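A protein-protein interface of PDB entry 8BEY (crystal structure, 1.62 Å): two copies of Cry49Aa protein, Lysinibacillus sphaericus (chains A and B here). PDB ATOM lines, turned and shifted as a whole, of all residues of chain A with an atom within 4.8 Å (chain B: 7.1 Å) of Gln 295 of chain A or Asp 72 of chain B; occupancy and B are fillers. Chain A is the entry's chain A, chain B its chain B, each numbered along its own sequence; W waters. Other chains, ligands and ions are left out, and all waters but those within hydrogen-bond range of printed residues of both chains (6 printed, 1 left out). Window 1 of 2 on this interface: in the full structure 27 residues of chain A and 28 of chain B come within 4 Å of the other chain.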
ATOM      1  N   ASP A  72       6.304  -8.814  33.589  1.00  0.00           N
ATOM      2  CA  ASP A  72       6.384  -7.795  32.516  1.00  0.00           C
ATOM      3  C   ASP A  72       7.812  -7.644  31.942  1.00  0.00           C
ATOM      4  O   ASP A  72       7.982  -7.149  30.762  1.00  0.00           O
ATOM      5  CB  ASP A  72       5.918  -6.431  33.042  1.00  0.00           C
ATOM      6  CG  ASP A  72       4.446  -6.293  33.406  1.00  0.00           C
ATOM      7  OD1 ASP A  72       3.625  -7.233  33.098  1.00  0.00           O
ATOM      8  OD2 ASP A  72       4.114  -5.220  34.011  1.00  0.00           O
ATOM      9  N   PHE A 293       3.440  -7.556  37.415  1.00  0.00           N
ATOM     10  CA  PHE A 293       2.461  -8.002  36.386  1.00  0.00           C
ATOM     11  C   PHE A 293       1.598  -6.833  35.889  1.00  0.00           C
ATOM     12  O   PHE A 293       0.605  -7.067  35.115  1.00  0.00           O
ATOM     13  CB  PHE A 293       1.533  -9.060  36.986  1.00  0.00           C
ATOM     14  CG  PHE A 293       2.248 -10.277  37.519  1.00  0.00           C
ATOM     15  CD1 PHE A 293       2.581 -11.311  36.663  1.00  0.00           C
ATOM     16  CD2 PHE A 293       2.597 -10.380  38.852  1.00  0.00           C
ATOM     17  CE1 PHE A 293       3.272 -12.429  37.128  1.00  0.00           C
ATOM     18  CE2 PHE A 293       3.266 -11.509  39.325  1.00  0.00           C
ATOM     19  CZ  PHE A 293       3.593 -12.538  38.461  1.00  0.00           C
ATOM     20  N   ARG A 294       1.921  -5.601  36.295  1.00  0.00           N
ATOM     21  CA  ARG A 294       0.961  -4.465  36.137  1.00  0.00           C
ATOM     22  C   ARG A 294       0.612  -4.206  34.665  1.00  0.00           C
ATOM     23  O   ARG A 294      -0.620  -3.927  34.395  1.00  0.00           O
ATOM     24  CB  ARG A 294       1.487  -3.205  36.834  1.00  0.00           C
ATOM     25  CG  ARG A 294       2.771  -2.626  36.262  1.00  0.00           C
ATOM     26  CD  ARG A 294       3.186  -1.317  36.938  1.00  0.00           C
ATOM     27  NE  ARG A 294       2.175  -0.327  36.604  1.00  0.00           N
ATOM     28  CZ  ARG A 294       1.642   0.597  37.423  1.00  0.00           C
ATOM     29  NH1 ARG A 294       2.063   0.757  38.672  1.00  0.00           N
ATOM     30  NH2 ARG A 294       0.692   1.391  36.953  1.00  0.00           N
ATOM     31  N   GLN A 295       1.572  -4.239  33.736  1.00  0.00           N
ATOM     32  CA  GLN A 295       1.283  -3.862  32.331  1.00  0.00           C
ATOM     33  C   GLN A 295       0.367  -4.924  31.706  1.00  0.00           C
ATOM     34  O   GLN A 295      -0.562  -4.547  30.910  1.00  0.00           O
ATOM     35  CB  GLN A 295       2.545  -3.599  31.502  1.00  0.00           C
ATOM     36  CG  GLN A 295       2.252  -2.930  30.171  1.00  0.00           C
ATOM     37  CD  GLN A 295       1.652  -1.549  30.337  1.00  0.00           C
ATOM     38  OE1 GLN A 295       2.211  -0.694  31.036  1.00  0.00           O
ATOM     39  NE2 GLN A 295       0.502  -1.312  29.712  1.00  0.00           N
ATOM     40  N   GLN A 296       0.618  -6.212  31.986  1.00  0.00           N
ATOM     41  CA  GLN A 296      -0.304  -7.289  31.513  1.00  0.00           C
ATOM     42  C   GLN A 296      -1.719  -7.075  32.070  1.00  0.00           C
ATOM     43  O   GLN A 296      -2.713  -7.239  31.296  1.00  0.00           O
ATOM     44  CB  GLN A 296       0.248  -8.654  31.933  1.00  0.00           C
ATOM     45  CG  GLN A 296       1.524  -8.994  31.199  1.00  0.00           C
ATOM     46  CD  GLN A 296       2.141 -10.242  31.785  1.00  0.00           C
ATOM     47  OE1 GLN A 296       1.724 -11.380  31.471  1.00  0.00           O
ATOM     48  NE2 GLN A 296       3.146 -10.040  32.626  1.00  0.00           N
ATOM     49  N   ILE A 297      -1.835  -6.745  33.351  1.00  0.00           N
ATOM     50  CA  ILE A 297      -3.145  -6.535  34.025  1.00  0.00           C
ATOM     51  C   ILE A 297      -3.882  -5.380  33.347  1.00  0.00           C
ATOM     52  O   ILE A 297      -5.110  -5.545  32.977  1.00  0.00           O
ATOM     53  CB  ILE A 297      -2.981  -6.403  35.552  1.00  0.00           C
ATOM     54  CG1 ILE A 297      -2.571  -7.760  36.147  1.00  0.00           C
ATOM     55  CG2 ILE A 297      -4.263  -5.864  36.170  1.00  0.00           C
ATOM     56  CD1 ILE A 297      -2.115  -7.724  37.585  1.00  0.00           C
ATOM     57  N   ILE A 298      -3.196  -4.250  33.161  1.00  0.00           N
ATOM     58  CA  ILE A 298      -3.778  -3.044  32.502  1.00  0.00           C
ATOM     59  C   ILE A 298      -4.213  -3.375  31.079  1.00  0.00           C
ATOM     60  O   ILE A 298      -5.376  -3.018  30.674  1.00  0.00           O
ATOM     61  CB  ILE A 298      -2.736  -1.904  32.542  1.00  0.00           C
ATOM     62  CG1 ILE A 298      -2.656  -1.345  33.963  1.00  0.00           C
ATOM     63  CG2 ILE A 298      -3.034  -0.848  31.499  1.00  0.00           C
ATOM     64  CD1 ILE A 298      -1.376  -0.601  34.223  1.00  0.00           C
ATOM     65  N   ASP A 299      -3.331  -4.039  30.310  1.00  0.00           N
ATOM     66  CA  ASP A 299      -3.578  -4.277  28.870  1.00  0.00           C
ATOM     67  C   ASP A 299      -4.808  -5.176  28.734  1.00  0.00           C
ATOM     68  O   ASP A 299      -5.640  -4.923  27.803  1.00  0.00           O
ATOM     69  CB  ASP A 299      -2.340  -4.837  28.162  1.00  0.00           C
ATOM     70  CG  ASP A 299      -1.239  -3.817  27.924  1.00  0.00           C
ATOM     71  OD1 ASP A 299      -1.542  -2.562  28.020  1.00  0.00           O
ATOM     72  OD2 ASP A 299      -0.108  -4.241  27.645  1.00  0.00           O
ATOM     73  N   ASN B   3      -5.322   1.817  25.262  1.00  0.00           N
ATOM     74  CA  ASN B   3      -5.015   1.845  26.717  1.00  0.00           C
ATOM     75  C   ASN B   3      -3.825   2.759  26.961  1.00  0.00           C
ATOM     76  O   ASN B   3      -2.809   2.276  27.513  1.00  0.00           O
ATOM     77  CB  ASN B   3      -4.746   0.450  27.285  1.00  0.00           C
ATOM     78  CG  ASN B   3      -6.022  -0.344  27.416  1.00  0.00           C
ATOM     79  OD1 ASN B   3      -7.059   0.212  27.785  1.00  0.00           O
ATOM     80  ND2 ASN B   3      -5.966  -1.628  27.078  1.00  0.00           N
ATOM     81  N   LEU B   4      -3.941   4.033  26.571  1.00  0.00           N
ATOM     82  CA  LEU B   4      -2.894   5.030  26.868  1.00  0.00           C
ATOM     83  C   LEU B   4      -3.495   6.146  27.708  1.00  0.00           C
ATOM     84  O   LEU B   4      -4.657   6.535  27.537  1.00  0.00           O
ATOM     85  CB  LEU B   4      -2.276   5.594  25.587  1.00  0.00           C
ATOM     86  CG  LEU B   4      -1.340   4.660  24.818  1.00  0.00           C
ATOM     87  CD1 LEU B   4      -0.978   5.290  23.480  1.00  0.00           C
ATOM     88  CD2 LEU B   4      -0.080   4.375  25.614  1.00  0.00           C
ATOM     89  N   ALA B  70       4.521   6.505  27.483  1.00  0.00           N
ATOM     90  CA  ALA B  70       4.223   5.652  28.653  1.00  0.00           C
ATOM     91  C   ALA B  70       5.115   4.410  28.612  1.00  0.00           C
ATOM     92  O   ALA B  70       5.028   3.601  27.615  1.00  0.00           O
ATOM     93  CB  ALA B  70       2.769   5.274  28.687  1.00  0.00           C
ATOM     94  N   LEU B  71       5.930   4.229  29.650  1.00  0.00           N
ATOM     95  CA  LEU B  71       6.770   3.002  29.830  1.00  0.00           C
ATOM     96  C   LEU B  71       5.949   1.914  30.516  1.00  0.00           C
ATOM     97  O   LEU B  71       4.946   2.225  31.264  1.00  0.00           O
ATOM     98  CB  LEU B  71       7.997   3.363  30.680  1.00  0.00           C
ATOM     99  CG  LEU B  71       8.840   4.524  30.155  1.00  0.00           C
ATOM    100  CD1 LEU B  71      10.020   4.786  31.066  1.00  0.00           C
ATOM    101  CD2 LEU B  71       9.321   4.249  28.754  1.00  0.00           C
ATOM    102  N   ASP B  72       6.396   0.648  30.385  1.00  0.00           N
ATOM    103  CA  ASP B  72       5.746  -0.499  31.051  1.00  0.00           C
ATOM    104  C   ASP B  72       5.706  -0.329  32.581  1.00  0.00           C
ATOM    105  O   ASP B  72       4.831  -0.954  33.257  1.00  0.00           O
ATOM    106  CB  ASP B  72       6.508  -1.791  30.714  1.00  0.00           C
ATOM    107  CG  ASP B  72       6.435  -2.270  29.268  1.00  0.00           C
ATOM    108  OD1 ASP B  72       5.617  -1.692  28.461  1.00  0.00           O
ATOM    109  OD2 ASP B  72       7.215  -3.238  28.957  1.00  0.00           O
ATOM    110  N   ASN B  73       6.663   0.400  33.158  1.00  0.00           N
ATOM    111  CA  ASN B  73       6.772   0.570  34.636  1.00  0.00           C
ATOM    112  C   ASN B  73       5.953   1.778  35.133  1.00  0.00           C
ATOM    113  O   ASN B  73       6.049   2.111  36.352  1.00  0.00           O
ATOM    114  CB  ASN B  73       8.228   0.683  35.085  1.00  0.00           C
ATOM    115  CG  ASN B  73       8.947   1.898  34.534  1.00  0.00           C
ATOM    116  OD1 ASN B  73       8.346   2.838  33.979  1.00  0.00           O
ATOM    117  ND2 ASN B  73      10.266   1.894  34.698  1.00  0.00           N
ATOM    118  N   ASN B  74       5.170   2.408  34.266  1.00  0.00           N
ATOM    119  CA  ASN B  74       4.195   3.487  34.622  1.00  0.00           C
ATOM    120  C   ASN B  74       4.911   4.833  34.748  1.00  0.00           C
ATOM    121  O   ASN B  74       4.206   5.872  35.105  1.00  0.00           O
ATOM    122  CB  ASN B  74       3.419   3.211  35.909  1.00  0.00           C
ATOM    123  CG  ASN B  74       2.113   3.983  35.955  1.00  0.00           C
ATOM    124  OD1 ASN B  74       1.400   4.034  34.950  1.00  0.00           O
ATOM    125  ND2 ASN B  74       1.787   4.574  37.095  1.00  0.00           N
ATOM    126  N   ASN B  75       6.210   4.875  34.461  1.00  0.00           N
ATOM    127  CA  ASN B  75       6.930   6.159  34.280  1.00  0.00           C
ATOM    128  C   ASN B  75       6.787   6.632  32.836  1.00  0.00           C
ATOM    129  O   ASN B  75       6.198   5.896  31.953  1.00  0.00           O
ATOM    130  CB  ASN B  75       8.393   6.041  34.705  1.00  0.00           C
ATOM    131  CG  ASN B  75       8.542   5.705  36.164  1.00  0.00           C
ATOM    132  OD1 ASN B  75       9.483   4.996  36.525  1.00  0.00           O
ATOM    133  ND2 ASN B  75       7.586   6.088  36.998  1.00  0.00           N
ATOM    134  N   SER B 290      14.170  -0.378  22.735  1.00  0.00           N
ATOM    135  CA  SER B 290      12.748  -0.820  22.688  1.00  0.00           C
ATOM    136  C   SER B 290      12.328  -1.514  23.995  1.00  0.00           C
ATOM    137  O   SER B 290      11.087  -1.601  24.284  1.00  0.00           O
ATOM    138  CB  SER B 290      12.547  -1.725  21.489  1.00  0.00           C
ATOM    139  OG  SER B 290      13.432  -2.859  21.589  1.00  0.00           O
ATOM    140  N   THR B 291      13.293  -2.044  24.764  1.00  0.00           N
ATOM    141  CA  THR B 291      13.043  -2.805  26.026  1.00  0.00           C
ATOM    142  C   THR B 291      12.031  -2.117  26.956  1.00  0.00           C
ATOM    143  O   THR B 291      11.214  -2.814  27.600  1.00  0.00           O
ATOM    144  CB  THR B 291      14.377  -3.138  26.722  1.00  0.00           C
ATOM    145  OG1 THR B 291      14.837  -4.308  26.031  1.00  0.00           O
ATOM    146  CG2 THR B 291      14.275  -3.412  28.202  1.00  0.00           C
ATOM    147  N   PRO B 292      12.092  -0.778  27.208  1.00  0.00           N
ATOM    148  CA  PRO B 292      11.191  -0.163  28.193  1.00  0.00           C
ATOM    149  C   PRO B 292       9.687  -0.229  27.848  1.00  0.00           C
ATOM    150  O   PRO B 292       8.817   0.043  28.751  1.00  0.00           O
ATOM    151  CB  PRO B 292      11.634   1.318  28.212  1.00  0.00           C
ATOM    152  CG  PRO B 292      13.071   1.284  27.721  1.00  0.00           C
ATOM    153  CD  PRO B 292      13.090   0.176  26.690  1.00  0.00           C
ATOM    154  N   PHE B 293       9.388  -0.584  26.591  1.00  0.00           N
ATOM    155  CA  PHE B 293       8.021  -0.667  26.012  1.00  0.00           C
ATOM    156  C   PHE B 293       7.636  -2.110  25.668  1.00  0.00           C
ATOM    157  O   PHE B 293       6.545  -2.325  25.032  1.00  0.00           O
ATOM    158  CB  PHE B 293       7.962   0.169  24.726  1.00  0.00           C
ATOM    159  CG  PHE B 293       8.310   1.625  24.940  1.00  0.00           C
ATOM    160  CD1 PHE B 293       7.348   2.522  25.349  1.00  0.00           C
ATOM    161  CD2 PHE B 293       9.594   2.089  24.713  1.00  0.00           C
ATOM    162  CE1 PHE B 293       7.660   3.865  25.571  1.00  0.00           C
ATOM    163  CE2 PHE B 293       9.912   3.429  24.934  1.00  0.00           C
ATOM    164  CZ  PHE B 293       8.944   4.319  25.353  1.00  0.00           C
ATOM    165  N   ARG B 294       8.460  -3.094  26.043  1.00  0.00           N
ATOM    166  CA  ARG B 294       8.333  -4.453  25.438  1.00  0.00           C
ATOM    167  C   ARG B 294       6.979  -5.111  25.769  1.00  0.00           C
ATOM    168  O   ARG B 294       6.412  -5.786  24.840  1.00  0.00           O
ATOM    169  CB  ARG B 294       9.521  -5.326  25.857  1.00  0.00           C
ATOM    170  CG  ARG B 294       9.639  -5.614  27.343  1.00  0.00           C
ATOM    171  CD  ARG B 294      10.817  -6.546  27.580  1.00  0.00           C
ATOM    172  NE  ARG B 294      10.478  -7.841  27.016  1.00  0.00           N
ATOM    173  CZ  ARG B 294      11.350  -8.718  26.555  1.00  0.00           C
ATOM    174  NH1 ARG B 294      10.905  -9.845  26.049  1.00  0.00           N
ATOM    175  NH2 ARG B 294      12.645  -8.466  26.566  1.00  0.00           N
ATOM    176  N   GLN B 295       6.444  -4.971  26.986  1.00  0.00           N
ATOM    177  CA  GLN B 295       5.186  -5.677  27.349  1.00  0.00           C
ATOM    178  C   GLN B 295       4.009  -5.070  26.572  1.00  0.00           C
ATOM    179  O   GLN B 295       3.110  -5.845  26.117  1.00  0.00           O
ATOM    180  CB  GLN B 295       4.944  -5.751  28.855  1.00  0.00           C
ATOM    181  CG  GLN B 295       3.833  -6.724  29.229  1.00  0.00           C
ATOM    182  CD  GLN B 295       4.214  -8.150  28.901  1.00  0.00           C
ATOM    183  OE1 GLN B 295       5.278  -8.632  29.331  1.00  0.00           O
ATOM    184  NE2 GLN B 295       3.361  -8.821  28.122  1.00  0.00           N
ATOM    185  N   GLN B 296       3.980  -3.740  26.402  1.00  0.00           N
ATOM    186  CA  GLN B 296       2.936  -3.101  25.549  1.00  0.00           C
ATOM    187  C   GLN B 296       3.051  -3.606  24.112  1.00  0.00           C
ATOM    188  O   GLN B 296       1.972  -3.884  23.470  1.00  0.00           O
ATOM    189  CB  GLN B 296       3.089  -1.577  25.598  1.00  0.00           C
ATOM    190  CG  GLN B 296       2.714  -1.015  26.936  1.00  0.00           C
ATOM    191  CD  GLN B 296       3.067   0.449  27.028  1.00  0.00           C
ATOM    192  OE1 GLN B 296       2.296   1.329  26.577  1.00  0.00           O
ATOM    193  NE2 GLN B 296       4.210   0.710  27.648  1.00  0.00           N
ATOM    194  N   ILE B 297       4.269  -3.699  23.582  1.00  0.00           N
ATOM    195  CA  ILE B 297       4.501  -4.127  22.173  1.00  0.00           C
ATOM    196  C   ILE B 297       3.980  -5.561  22.017  1.00  0.00           C
ATOM    197  O   ILE B 297       3.218  -5.845  21.021  1.00  0.00           O
ATOM    198  CB  ILE B 297       5.978  -3.929  21.770  1.00  0.00           C
ATOM    199  CG1 ILE B 297       6.265  -2.427  21.647  1.00  0.00           C
ATOM    200  CG2 ILE B 297       6.284  -4.687  20.489  1.00  0.00           C
ATOM    201  CD1 ILE B 297       7.718  -2.061  21.504  1.00  0.00           C
ATOM    202  N   ASP B 299       1.823  -7.261  23.953  1.00  0.00           N
ATOM    203  CA  ASP B 299       0.372  -7.389  24.235  1.00  0.00           C
ATOM    204  C   ASP B 299      -0.420  -6.922  23.009  1.00  0.00           C
ATOM    205  O   ASP B 299      -1.435  -7.573  22.670  1.00  0.00           O
ATOM    206  CB  ASP B 299      -0.030  -6.634  25.500  1.00  0.00           C
ATOM    207  CG  ASP B 299       0.424  -7.279  26.797  1.00  0.00           C
ATOM    208  OD1 ASP B 299       0.759  -8.515  26.747  1.00  0.00           O
ATOM    209  OD2 ASP B 299       0.376  -6.582  27.845  1.00  0.00           O
ATOM    210  N   ASN B 300      -0.014  -5.821  22.378  1.00  0.00           N
ATOM    211  CA  ASN B 300      -0.816  -5.196  21.296  1.00  0.00           C
ATOM    212  C   ASN B 300      -0.519  -5.853  19.954  1.00  0.00           C
ATOM    213  O   ASN B 300      -1.496  -5.990  19.135  1.00  0.00           O
ATOM    214  CB  ASN B 300      -0.604  -3.679  21.300  1.00  0.00           C
ATOM    215  CG  ASN B 300      -1.292  -3.078  22.508  1.00  0.00           C
ATOM    216  OD1 ASN B 300      -2.497  -3.217  22.712  1.00  0.00           O
ATOM    217  ND2 ASN B 300      -0.528  -2.459  23.368  1.00  0.00           N
HETATM  218  O   HOH W   1      -0.530   2.713  38.940  1.00  0.00           O
HETATM  219  O   HOH W   2       5.906  -3.251  34.392  1.00  0.00           O
HETATM  220  O   HOH W   3       2.170   0.037  33.932  1.00  0.00           O
HETATM  221  O   HOH W   4       2.089   2.107  30.898  1.00  0.00           O
HETATM  222  O   HOH W   5       8.629  -4.481  30.787  1.00  0.00           O
HETATM  223  O   HOH W   6      -1.413  -1.170  25.703  1.00  0.00           O
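Printed residues of chain B that touch a printed residue of chain A: Asn 3, Asp 72, Asn 74, Gln 295, Gln 296 and Asp 299.
Of the 8 printed residues of chain A, 6 touch a printed residue of chain B.
Among the printed residues, 12 pairs touch across the chains.
Among the printed residues, no Asp or Glu carboxylate lies within 4 Å of a Lys or Arg side-chain nitrogen of the other chain.
Gln 296 of chain B touches Gln 295 of chain A.
O of Gln 295 of chain A touches OD2 of Asp 299 of chain B (3.8 Å).
Gln 296 of chain A touches Gln 295 of chain B (CG to NE2, 3.6 Å).
CA of Gln 296 of chain A touches OD2 of Asp 299 of chain B, 3.8 Å away.
O of Ile 298 of chain A touches ND2 of Asn 3 of chain B, 3.9 Å away.
OD2 of Asp 299 of chain A touches O of Gln 295 of chain B (3.9 Å).
OD2 of Asp 299 of chain A touches CA of Gln 296 of chain B (3.9 Å).
Of the printed residues of chain A, Asp 72 of chain B touches Gln 295 (3.4 Å).
Of the printed residues of chain B, Asp 72 of chain A touches Gln 295.
Of the printed residues of chain B, Arg 294 of chain A touches Asn 74.
Of the printed residues of chain A, Asn 74 of chain B touches Arg 294 (3.1 Å).
Of the printed residues of chain A, Gln 295 of chain B touches Asp 72 (3.4 Å), Gln 296 (3.6 Å) and Asp 299 (3.9 Å).
Of the printed residues of chain A, Asp 299 of chain B touches Gln 295 (3.8 Å), Gln 296 (3.8 Å) and Asp 299 (2.4 Å).
Leu 71 of chain B touches none of the printed residues of chain A.
The nearest printed residue of chain B that does not touch Gln 295 of chain A is Leu 71 of chain B (4.01 Å).
The nearest printed residue of chain A that does not touch Asp 72 of chain B is Arg 294 of chain A (4.01 Å).
The nearest printed residue of chain B that does not touch Arg 294 of chain A is Asp 72 of chain B (4.01 Å).
N of Arg 294 of chain A is in hydrogen-bond range of OD2 of Asp 72 of chain A, 3.2 Å away.
OD2 of Asp 72 of chain A is in hydrogen-bond range of N of Gln 295 of chain A.
The side-chain amide nitrogen of Gln 296 of chain A is in hydrogen-bond range of the side-chain carboxylate of Asp 72 of chain A, 2.9 Å away.
The side-chain amide nitrogen (NE2) of Gln 295 of chain A is in hydrogen-bond range of the side-chain carboxylate (OD1) of Asp 299 of chain A, at 2.9 Å.
The side-chain carboxylate (OD2) of Asp 72 of chain B lies within hydrogen-bond range of the backbone NH (N) of Gln 295 of chain B, 2.7 Å away.
The side-chain carboxylate (OD1) of Asp 72 of chain B lies within hydrogen-bond range of the side-chain amide nitrogen (NE2) of Gln 296 of chain B, 2.9 Å away.
Asp 72 of chain A touches Gln 295 of chain B, and with the chains exchanged Gln 295 of chain A touches Asp 72 of chain B.
Gln 295 of chain A touches Gln 296 of chain B, and with the chains exchanged Gln 296 of chain A touches Gln 295 of chain B.
Gln 295 of chain A touches Asp 299 of chain B, and with the chains exchanged Asp 299 of chain A touches Gln 295 of chain B.
Gln 296 of chain A touches Asp 299 of chain B, and with the chains exchanged Asp 299 of chain A touches Gln 296 of chain B.
Positions printed for both chains: 72, 293, 294, 295, 296, 297 and 299.
OE1 of Gln 295 of chain B lies close to O of Asp 72 of chain A (3.4 Å).
The guanidinium group of Arg 294 of chain A lies close to the side-chain amide nitrogen of Asn 74 of chain B (3.4 Å).
OE1 of Gln 295 of chain A lies close to O of Asp 72 of chain B, 3.4 Å away.
O of Asp 299 of chain A lies within hydrogen-bond range of ND2 of Asn 3 of chain B.
The side-chain carboxylate (OD2) of Asp 299 of chain B lies close to the side-chain carboxylate (OD2) of Asp 299 of chain A.
Water W5 bridges the side-chain carboxylate (OD2) of Asp 72 of chain B (2.6 Å) and the backbone carbonyl oxygen (O) of Asp 72 of chain A (2.7 Å).
Water W1 bridges NH2 of Arg 294 of chain A (2.7 Å) and ND2 of Asn 74 of chain B (3.5 Å).
Water W2 lies within hydrogen-bond range of OD2 of Asp 72 of chain A (2.7 Å) and O of Asp 72 of chain B (2.8 Å).
Water W3 lies within hydrogen-bond range of NE of Arg 294 of chain A, O of Asp 72 of chain B and OE1 of Gln 295 of chain A.
Water W6 lies within hydrogen-bond range of OD1 of Asp 299 of chain A and ND2 of Asn 300 of chain B.
Water W4 bridges OE1 of Gln 295 of chain A (2.8 Å) and O of Leu 71 of chain B (2.9 Å).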
